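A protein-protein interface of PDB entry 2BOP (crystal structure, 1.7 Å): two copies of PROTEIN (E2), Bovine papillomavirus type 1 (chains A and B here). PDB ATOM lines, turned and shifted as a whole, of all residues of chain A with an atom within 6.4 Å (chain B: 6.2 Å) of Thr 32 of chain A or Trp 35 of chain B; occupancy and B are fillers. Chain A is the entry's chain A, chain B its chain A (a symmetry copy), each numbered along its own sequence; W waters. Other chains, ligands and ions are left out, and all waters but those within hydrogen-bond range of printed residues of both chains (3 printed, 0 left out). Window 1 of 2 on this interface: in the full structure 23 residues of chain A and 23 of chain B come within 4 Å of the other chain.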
ATOM      1  N   ARG A  17     -25.264 -23.355  36.868  1.00  0.00           N
ATOM      2  CA  ARG A  17     -23.954 -23.989  37.334  1.00  0.00           C
ATOM      3  C   ARG A  17     -23.721 -23.819  38.844  1.00  0.00           C
ATOM      4  O   ARG A  17     -23.351 -24.765  39.529  1.00  0.00           O
ATOM      5  CB  ARG A  17     -22.781 -23.385  36.563  1.00  0.00           C
ATOM      6  CG  ARG A  17     -21.396 -23.763  37.143  1.00  0.00           C
ATOM      7  CD  ARG A  17     -20.260 -23.415  36.198  1.00  0.00           C
ATOM      8  NE  ARG A  17     -20.045 -22.004  35.988  1.00  0.00           N
ATOM      9  CZ  ARG A  17     -20.233 -21.249  34.911  1.00  0.00           C
ATOM     10  NH1 ARG A  17     -20.694 -21.772  33.805  1.00  0.00           N
ATOM     11  NH2 ARG A  17     -20.238 -19.910  35.102  1.00  0.00           N
ATOM     12  N   ASN A  30     -17.508 -33.243  35.910  1.00  0.00           N
ATOM     13  CA  ASN A  30     -17.021 -31.883  35.826  1.00  0.00           C
ATOM     14  C   ASN A  30     -18.036 -31.022  35.058  1.00  0.00           C
ATOM     15  O   ASN A  30     -18.861 -31.581  34.281  1.00  0.00           O
ATOM     16  CB  ASN A  30     -15.651 -31.879  35.053  1.00  0.00           C
ATOM     17  CG  ASN A  30     -14.577 -32.192  36.074  1.00  0.00           C
ATOM     18  OD1 ASN A  30     -14.536 -31.636  37.214  1.00  0.00           O
ATOM     19  ND2 ASN A  30     -13.875 -33.253  35.699  1.00  0.00           N
ATOM     20  N   CYS A  31     -17.790 -29.728  35.108  1.00  0.00           N
ATOM     21  CA  CYS A  31     -18.684 -28.764  34.416  1.00  0.00           C
ATOM     22  C   CYS A  31     -17.748 -27.660  33.938  1.00  0.00           C
ATOM     23  O   CYS A  31     -16.672 -27.426  34.535  1.00  0.00           O
ATOM     24  CB  CYS A  31     -19.693 -28.229  35.476  1.00  0.00           C
ATOM     25  SG  CYS A  31     -20.836 -27.031  34.911  1.00  0.00           S
ATOM     26  N   THR A  32     -18.214 -26.957  32.889  1.00  0.00           N
ATOM     27  CA  THR A  32     -17.432 -25.862  32.287  1.00  0.00           C
ATOM     28  C   THR A  32     -17.937 -24.496  32.616  1.00  0.00           C
ATOM     29  O   THR A  32     -19.103 -24.378  33.101  1.00  0.00           O
ATOM     30  CB  THR A  32     -17.325 -26.006  30.710  1.00  0.00           C
ATOM     31  OG1 THR A  32     -18.653 -25.703  30.152  1.00  0.00           O
ATOM     32  CG2 THR A  32     -16.812 -27.384  30.296  1.00  0.00           C
ATOM     33  N   THR A  33     -17.150 -23.531  32.354  1.00  0.00           N
ATOM     34  CA  THR A  33     -17.602 -22.112  32.236  1.00  0.00           C
ATOM     35  C   THR A  33     -18.600 -22.029  31.069  1.00  0.00           C
ATOM     36  O   THR A  33     -18.719 -22.911  30.229  1.00  0.00           O
ATOM     37  CB  THR A  33     -16.407 -21.103  32.103  1.00  0.00           C
ATOM     38  OG1 THR A  33     -15.672 -21.466  30.918  1.00  0.00           O
ATOM     39  CG2 THR A  33     -15.526 -21.077  33.366  1.00  0.00           C
ATOM     40  N   THR A  34     -19.178 -20.854  30.941  1.00  0.00           N
ATOM     41  CA  THR A  34     -20.218 -20.610  29.912  1.00  0.00           C
ATOM     42  C   THR A  34     -19.538 -20.219  28.617  1.00  0.00           C
ATOM     43  O   THR A  34     -18.672 -19.318  28.564  1.00  0.00           O
ATOM     44  CB  THR A  34     -21.216 -19.464  30.349  1.00  0.00           C
ATOM     45  OG1 THR A  34     -21.631 -19.740  31.691  1.00  0.00           O
ATOM     46  CG2 THR A  34     -22.358 -19.273  29.375  1.00  0.00           C
ATOM     47  N   TRP A  35     -19.986 -20.857  27.513  1.00  0.00           N
ATOM     48  CA  TRP A  35     -19.429 -20.566  26.193  1.00  0.00           C
ATOM     49  C   TRP A  35     -20.469 -20.368  25.128  1.00  0.00           C
ATOM     50  O   TRP A  35     -21.665 -20.703  25.399  1.00  0.00           O
ATOM     51  CB  TRP A  35     -18.356 -21.576  25.810  1.00  0.00           C
ATOM     52  CG  TRP A  35     -18.788 -22.993  25.954  1.00  0.00           C
ATOM     53  CD1 TRP A  35     -18.650 -23.783  27.073  1.00  0.00           C
ATOM     54  CD2 TRP A  35     -19.440 -23.766  24.971  1.00  0.00           C
ATOM     55  NE1 TRP A  35     -19.049 -25.041  26.748  1.00  0.00           N
ATOM     56  CE2 TRP A  35     -19.611 -25.063  25.520  1.00  0.00           C
ATOM     57  CE3 TRP A  35     -19.780 -23.570  23.617  1.00  0.00           C
ATOM     58  CZ2 TRP A  35     -20.124 -26.121  24.756  1.00  0.00           C
ATOM     59  CZ3 TRP A  35     -20.269 -24.628  22.854  1.00  0.00           C
ATOM     60  CH2 TRP A  35     -20.443 -25.895  23.456  1.00  0.00           C
ATOM     61  N   PHE A  36     -20.078 -19.829  24.017  1.00  0.00           N
ATOM     62  CA  PHE A  36     -21.016 -19.628  22.848  1.00  0.00           C
ATOM     63  C   PHE A  36     -20.235 -20.068  21.570  1.00  0.00           C
ATOM     64  O   PHE A  36     -18.999 -19.997  21.593  1.00  0.00           O
ATOM     65  CB  PHE A  36     -21.190 -18.070  22.679  1.00  0.00           C
ATOM     66  CG  PHE A  36     -21.885 -17.438  23.839  1.00  0.00           C
ATOM     67  CD1 PHE A  36     -21.131 -17.064  24.960  1.00  0.00           C
ATOM     68  CD2 PHE A  36     -23.222 -17.219  23.784  1.00  0.00           C
ATOM     69  CE1 PHE A  36     -21.750 -16.410  26.062  1.00  0.00           C
ATOM     70  CE2 PHE A  36     -23.844 -16.501  24.882  1.00  0.00           C
ATOM     71  CZ  PHE A  36     -23.066 -16.190  25.933  1.00  0.00           C
ATOM     72  N   GLN A  50     -24.076 -21.916  26.531  1.00  0.00           N
ATOM     73  CA  GLN A  50     -23.960 -23.356  26.790  1.00  0.00           C
ATOM     74  C   GLN A  50     -22.994 -23.608  27.944  1.00  0.00           C
ATOM     75  O   GLN A  50     -22.067 -22.864  28.115  1.00  0.00           O
ATOM     76  CB  GLN A  50     -23.303 -24.130  25.619  1.00  0.00           C
ATOM     77  CG  GLN A  50     -23.793 -23.783  24.255  1.00  0.00           C
ATOM     78  CD  GLN A  50     -24.925 -24.645  23.829  1.00  0.00           C
ATOM     79  OE1 GLN A  50     -25.252 -25.669  24.438  1.00  0.00           O
ATOM     80  NE2 GLN A  50     -25.543 -24.344  22.710  1.00  0.00           N
ATOM     81  N   ILE A  51     -23.244 -24.708  28.648  1.00  0.00           N
ATOM     82  CA  ILE A  51     -22.251 -25.358  29.476  1.00  0.00           C
ATOM     83  C   ILE A  51     -22.165 -26.819  29.067  1.00  0.00           C
ATOM     84  O   ILE A  51     -23.140 -27.387  28.598  1.00  0.00           O
ATOM     85  CB  ILE A  51     -22.383 -25.211  31.015  1.00  0.00           C
ATOM     86  CG1 ILE A  51     -23.797 -25.710  31.424  1.00  0.00           C
ATOM     87  CG2 ILE A  51     -22.161 -23.659  31.387  1.00  0.00           C
ATOM     88  CD1 ILE A  51     -23.756 -25.856  33.035  1.00  0.00           C
ATOM     89  N   LEU A  52     -20.963 -27.384  29.254  1.00  0.00           N
ATOM     90  CA  LEU A  52     -20.787 -28.856  29.062  1.00  0.00           C
ATOM     91  C   LEU A  52     -20.615 -29.494  30.448  1.00  0.00           C
ATOM     92  O   LEU A  52     -19.914 -28.942  31.322  1.00  0.00           O
ATOM     93  CB  LEU A  52     -19.559 -28.981  28.193  1.00  0.00           C
ATOM     94  CG  LEU A  52     -19.512 -30.346  27.424  1.00  0.00           C
ATOM     95  CD1 LEU A  52     -18.762 -30.178  26.131  1.00  0.00           C
ATOM     96  CD2 LEU A  52     -18.721 -31.210  28.431  1.00  0.00           C
ATOM     97  N   ILE A  53     -21.310 -30.543  30.705  1.00  0.00           N
ATOM     98  CA  ILE A  53     -21.256 -31.356  31.916  1.00  0.00           C
ATOM     99  C   ILE A  53     -20.830 -32.768  31.525  1.00  0.00           C
ATOM    100  O   ILE A  53     -21.463 -33.389  30.635  1.00  0.00           O
ATOM    101  CB  ILE A  53     -22.640 -31.320  32.689  1.00  0.00           C
ATOM    102  CG1 ILE A  53     -22.924 -29.867  33.081  1.00  0.00           C
ATOM    103  CG2 ILE A  53     -22.473 -32.225  33.988  1.00  0.00           C
ATOM    104  CD1 ILE A  53     -23.803 -29.720  34.375  1.00  0.00           C
ATOM    105  N   LEU B   5     -10.917 -30.489  20.081  1.00  0.00           N
ATOM    106  CA  LEU B   5     -10.658 -29.631  21.279  1.00  0.00           C
ATOM    107  C   LEU B   5      -9.222 -29.129  21.171  1.00  0.00           C
ATOM    108  O   LEU B   5      -8.328 -29.975  20.948  1.00  0.00           O
ATOM    109  CB  LEU B   5     -10.819 -30.521  22.501  1.00  0.00           C
ATOM    110  CG  LEU B   5     -11.686 -30.130  23.590  1.00  0.00           C
ATOM    111  CD1 LEU B   5     -13.022 -29.525  23.050  1.00  0.00           C
ATOM    112  CD2 LEU B   5     -12.080 -31.442  24.297  1.00  0.00           C
ATOM    113  N   THR B  32     -15.871 -22.052  19.096  1.00  0.00           N
ATOM    114  CA  THR B  32     -16.426 -21.472  20.333  1.00  0.00           C
ATOM    115  C   THR B  32     -15.590 -20.390  20.930  1.00  0.00           C
ATOM    116  O   THR B  32     -14.391 -20.260  20.539  1.00  0.00           O
ATOM    117  CB  THR B  32     -16.703 -22.580  21.436  1.00  0.00           C
ATOM    118  OG1 THR B  32     -15.395 -23.034  21.937  1.00  0.00           O
ATOM    119  CG2 THR B  32     -17.558 -23.724  20.895  1.00  0.00           C
ATOM    120  N   THR B  33     -16.151 -19.681  21.826  1.00  0.00           N
ATOM    121  CA  THR B  33     -15.393 -18.839  22.800  1.00  0.00           C
ATOM    122  C   THR B  33     -14.509 -19.772  23.646  1.00  0.00           C
ATOM    123  O   THR B  33     -14.674 -20.984  23.692  1.00  0.00           O
ATOM    124  CB  THR B  33     -16.327 -17.919  23.664  1.00  0.00           C
ATOM    125  OG1 THR B  33     -17.228 -18.782  24.385  1.00  0.00           O
ATOM    126  CG2 THR B  33     -17.062 -16.871  22.807  1.00  0.00           C
ATOM    127  N   THR B  34     -13.687 -19.142  24.457  1.00  0.00           N
ATOM    128  CA  THR B  34     -12.714 -19.879  25.299  1.00  0.00           C
ATOM    129  C   THR B  34     -13.395 -20.283  26.589  1.00  0.00           C
ATOM    130  O   THR B  34     -14.029 -19.465  27.293  1.00  0.00           O
ATOM    131  CB  THR B  34     -11.442 -19.000  25.628  1.00  0.00           C
ATOM    132  OG1 THR B  34     -10.986 -18.421  24.402  1.00  0.00           O
ATOM    133  CG2 THR B  34     -10.377 -19.764  26.386  1.00  0.00           C
ATOM    134  N   TRP B  35     -13.209 -21.568  26.966  1.00  0.00           N
ATOM    135  CA  TRP B  35     -13.796 -22.089  28.198  1.00  0.00           C
ATOM    136  C   TRP B  35     -12.837 -22.881  29.038  1.00  0.00           C
ATOM    137  O   TRP B  35     -11.733 -23.225  28.510  1.00  0.00           O
ATOM    138  CB  TRP B  35     -15.104 -22.817  27.924  1.00  0.00           C
ATOM    139  CG  TRP B  35     -15.004 -23.846  26.853  1.00  0.00           C
ATOM    140  CD1 TRP B  35     -15.223 -23.654  25.508  1.00  0.00           C
ATOM    141  CD2 TRP B  35     -14.639 -25.196  27.032  1.00  0.00           C
ATOM    142  NE1 TRP B  35     -15.158 -24.868  24.897  1.00  0.00           N
ATOM    143  CE2 TRP B  35     -14.727 -25.815  25.758  1.00  0.00           C
ATOM    144  CE3 TRP B  35     -14.383 -26.017  28.150  1.00  0.00           C
ATOM    145  CZ2 TRP B  35     -14.544 -27.195  25.598  1.00  0.00           C
ATOM    146  CZ3 TRP B  35     -14.224 -27.392  27.992  1.00  0.00           C
ATOM    147  CH2 TRP B  35     -14.297 -27.954  26.697  1.00  0.00           C
ATOM    148  N   PHE B  36     -13.188 -23.125  30.261  1.00  0.00           N
ATOM    149  CA  PHE B  36     -12.336 -23.961  31.189  1.00  0.00           C
ATOM    150  C   PHE B  36     -13.307 -24.929  31.935  1.00  0.00           C
ATOM    151  O   PHE B  36     -14.486 -24.575  32.072  1.00  0.00           O
ATOM    152  CB  PHE B  36     -11.819 -22.987  32.317  1.00  0.00           C
ATOM    153  CG  PHE B  36     -10.896 -21.936  31.794  1.00  0.00           C
ATOM    154  CD1 PHE B  36     -11.440 -20.760  31.259  1.00  0.00           C
ATOM    155  CD2 PHE B  36      -9.555 -22.127  31.860  1.00  0.00           C
ATOM    156  CE1 PHE B  36     -10.592 -19.715  30.802  1.00  0.00           C
ATOM    157  CE2 PHE B  36      -8.688 -21.038  31.446  1.00  0.00           C
ATOM    158  CZ  PHE B  36      -9.277 -19.947  30.926  1.00  0.00           C
ATOM    159  N   THR B  37     -12.698 -25.950  32.455  1.00  0.00           N
ATOM    160  CA  THR B  37     -13.431 -26.839  33.433  1.00  0.00           C
ATOM    161  C   THR B  37     -13.293 -26.116  34.759  1.00  0.00           C
ATOM    162  O   THR B  37     -12.218 -25.576  35.083  1.00  0.00           O
ATOM    163  CB  THR B  37     -12.670 -28.222  33.505  1.00  0.00           C
ATOM    164  OG1 THR B  37     -12.899 -28.816  32.194  1.00  0.00           O
ATOM    165  CG2 THR B  37     -13.323 -29.157  34.571  1.00  0.00           C
ATOM    166  N   VAL B  38     -14.361 -25.926  35.528  1.00  0.00           N
ATOM    167  CA  VAL B  38     -14.266 -25.193  36.798  1.00  0.00           C
ATOM    168  C   VAL B  38     -13.742 -26.135  37.913  1.00  0.00           C
ATOM    169  O   VAL B  38     -13.949 -27.330  37.822  1.00  0.00           O
ATOM    170  CB  VAL B  38     -15.622 -24.566  37.178  1.00  0.00           C
ATOM    171  CG1 VAL B  38     -16.148 -23.612  36.120  1.00  0.00           C
ATOM    172  CG2 VAL B  38     -16.619 -25.655  37.597  1.00  0.00           C
ATOM    173  N   GLN B  48      -6.088 -26.457  31.286  1.00  0.00           N
ATOM    174  CA  GLN B  48      -5.796 -25.367  30.277  1.00  0.00           C
ATOM    175  C   GLN B  48      -7.047 -24.853  29.678  1.00  0.00           C
ATOM    176  O   GLN B  48      -8.139 -25.444  29.815  1.00  0.00           O
ATOM    177  CB  GLN B  48      -4.884 -25.933  29.170  1.00  0.00           C
ATOM    178  CG  GLN B  48      -3.410 -26.084  29.657  1.00  0.00           C
ATOM    179  CD  GLN B  48      -2.758 -26.901  28.555  1.00  0.00           C
ATOM    180  OE1 GLN B  48      -1.964 -26.412  27.758  1.00  0.00           O
ATOM    181  NE2 GLN B  48      -3.343 -28.086  28.319  1.00  0.00           N
ATOM    182  N   ALA B  49      -6.961 -23.631  29.085  1.00  0.00           N
ATOM    183  CA  ALA B  49      -8.038 -23.059  28.298  1.00  0.00           C
ATOM    184  C   ALA B  49      -8.301 -23.918  27.072  1.00  0.00           C
ATOM    185  O   ALA B  49      -7.398 -24.550  26.487  1.00  0.00           O
ATOM    186  CB  ALA B  49      -7.668 -21.610  27.925  1.00  0.00           C
ATOM    187  N   GLN B  50      -9.581 -23.925  26.654  1.00  0.00           N
ATOM    188  CA  GLN B  50     -10.005 -24.768  25.530  1.00  0.00           C
ATOM    189  C   GLN B  50     -10.898 -23.972  24.582  1.00  0.00           C
ATOM    190  O   GLN B  50     -11.607 -23.109  25.020  1.00  0.00           O
ATOM    191  CB  GLN B  50     -10.925 -25.936  25.966  1.00  0.00           C
ATOM    192  CG  GLN B  50     -10.490 -26.690  27.176  1.00  0.00           C
ATOM    193  CD  GLN B  50      -9.633 -27.853  26.836  1.00  0.00           C
ATOM    194  OE1 GLN B  50      -9.500 -28.271  25.681  1.00  0.00           O
ATOM    195  NE2 GLN B  50      -9.062 -28.510  27.820  1.00  0.00           N
ATOM    196  N   ILE B  51     -10.851 -24.365  23.313  1.00  0.00           N
ATOM    197  CA  ILE B  51     -11.890 -24.064  22.354  1.00  0.00           C
ATOM    198  C   ILE B  51     -12.350 -25.365  21.716  1.00  0.00           C
ATOM    199  O   ILE B  51     -11.579 -26.308  21.613  1.00  0.00           O
ATOM    200  CB  ILE B  51     -11.593 -22.985  21.278  1.00  0.00           C
ATOM    201  CG1 ILE B  51     -10.303 -23.409  20.520  1.00  0.00           C
ATOM    202  CG2 ILE B  51     -11.412 -21.571  22.029  1.00  0.00           C
ATOM    203  CD1 ILE B  51     -10.235 -22.454  19.216  1.00  0.00           C
ATOM    204  N   LEU B  52     -13.629 -25.371  21.313  1.00  0.00           N
ATOM    205  CA  LEU B  52     -14.159 -26.517  20.514  1.00  0.00           C
ATOM    206  C   LEU B  52     -14.352 -26.034  19.069  1.00  0.00           C
ATOM    207  O   LEU B  52     -14.826 -24.902  18.833  1.00  0.00           O
ATOM    208  CB  LEU B  52     -15.454 -26.887  21.196  1.00  0.00           C
ATOM    209  CG  LEU B  52     -15.886 -28.363  20.889  1.00  0.00           C
ATOM    210  CD1 LEU B  52     -16.687 -28.909  22.039  1.00  0.00           C
ATOM    211  CD2 LEU B  52     -16.765 -28.146  19.637  1.00  0.00           C
HETATM  212  O   HOH W   1     -16.654 -18.414  26.945  1.00  0.00           O
HETATM  213  O   HOH W   2     -15.915 -19.398  29.279  1.00  0.00           O
HETATM  214  O   HOH W   3     -15.821 -29.206  37.367  1.00  0.00           O
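N of Val 38 of chain B lies within hydrogen-bond range of O of Cys 31 of chain A (2.9 Å).
The backbone NH of Thr 33 of chain A is in hydrogen-bond range of the backbone carbonyl oxygen of Phe 36 of chain B.
The backbone carbonyl oxygen of Phe 36 of chain A lies within hydrogen-bond range of the backbone NH of Thr 33 of chain B, at 2.9 Å.
NH1 of Arg 17 of chain A sits at hydrogen-bond distance from O of Thr 32 of chain A.
OG1 of Thr 32 of chain A sits at hydrogen-bond distance from N of Leu 52 of chain A.
The backbone NH (N) of Gln 50 of chain A sits at hydrogen-bond distance from the backbone carbonyl oxygen (O) of Trp 35 of chain A, at 2.9 Å.
The side-chain hydroxyl (OG1) of Thr 32 of chain B sits at hydrogen-bond distance from the indole nitrogen (NE1) of Trp 35 of chain B (3.5 Å).
The backbone NH (N) of Leu 52 of chain B lies within hydrogen-bond range of the side-chain hydroxyl (OG1) of Thr 32 of chain B (3.0 Å).
The backbone carbonyl oxygen of Trp 35 of chain B lies within hydrogen-bond range of the backbone NH of Gln 50 of chain B (2.9 Å).
Asn 30 of chain A touches Thr 37 of chain B.
O of Cys 31 of chain A touches CA of Thr 37 of chain B, at 3.5 Å.
Trp 35 of chain B touches Thr 32 of chain A (CZ3 to CG2, 3.5 Å).
O of Phe 36 of chain B touches CA of Thr 32 of chain A, at 3.2 Å.
Thr 33 of chain A touches Trp 35 of chain B.
CG2 of Thr 33 of chain A touches CG1 of Val 38 of chain B, 3.8 Å away.
Thr 32 of chain B touches Trp 35 of chain A.
Trp 35 of chain A touches Thr 33 of chain B.
CD1 of Trp 35 of chain B touches CG of Trp 35 of chain A, 3.7 Å away.
Phe 36 of chain A touches Thr 32 of chain B.
Of the printed residues of chain A, Thr 33 of chain B touches Trp 35 and Phe 36.
Trp 35 of chain B touches three residues of chain A.
Of the printed residues of chain A, Thr 37 of chain B touches Asn 30 (3.6 Å) and Cys 31 (3.5 Å).
The nearest residue of chain B that does not touch Thr 32 of chain A is Val 38 of chain B (4.03 Å).
The nearest printed residue of chain A that does not touch Trp 35 of chain B is Leu 52 of chain A (5.0 Å).
The nearest printed residue of chain B that does not touch Cys 31 of chain A is Phe 36 of chain B (4.4 Å).
Printed residues of chain A that touch a printed residue of chain B: Asn 30, Cys 31, Thr 32, Thr 33, Trp 35 and Phe 36.
Of the 13 printed residues of chain B, 6 touch a printed residue of chain A.
Printed residues of chain B that touch a printed residue of chain A: Thr 32, Thr 33, Trp 35, Phe 36, Thr 37 and Val 38.
Hydrophobic or aromatic side chains of chain B that line the printed part of chain A: Trp 35 and Val 38.
Thr 32 of chain A touches Trp 35 of chain B, and with the chains exchanged Trp 35 of chain A touches Thr 32 of chain B.
Thr 33 of chain A touches Trp 35 of chain B, and with the chains exchanged Trp 35 of chain A touches Thr 33 of chain B.
Thr 33 of chain A touches Phe 36 of chain B, and with the chains exchanged Phe 36 of chain A touches Thr 33 of chain B.
Trp 35 of chain B touches its own counterpart, Trp 35 of chain A.
Water W1 lies within hydrogen-bond range of the side-chain hydroxyl of Thr 33 of chain B, the backbone carbonyl oxygen of Thr 34 of chain A and the backbone carbonyl oxygen of Thr 34 of chain B.
Water W2 lies within hydrogen-bond range of OG1 of Thr 33 of chain A (2.6 Å), O of Thr 34 of chain B (2.7 Å) and O of Thr 34 of chain A (2.8 Å).
Water W3 lies within hydrogen-bond range of the backbone carbonyl oxygen of Val 38 of chain B (2.7 Å), the side-chain amide oxygen of Asn 30 of chain A (2.8 Å) and the backbone NH of Cys 31 of chain A (3.0 Å).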
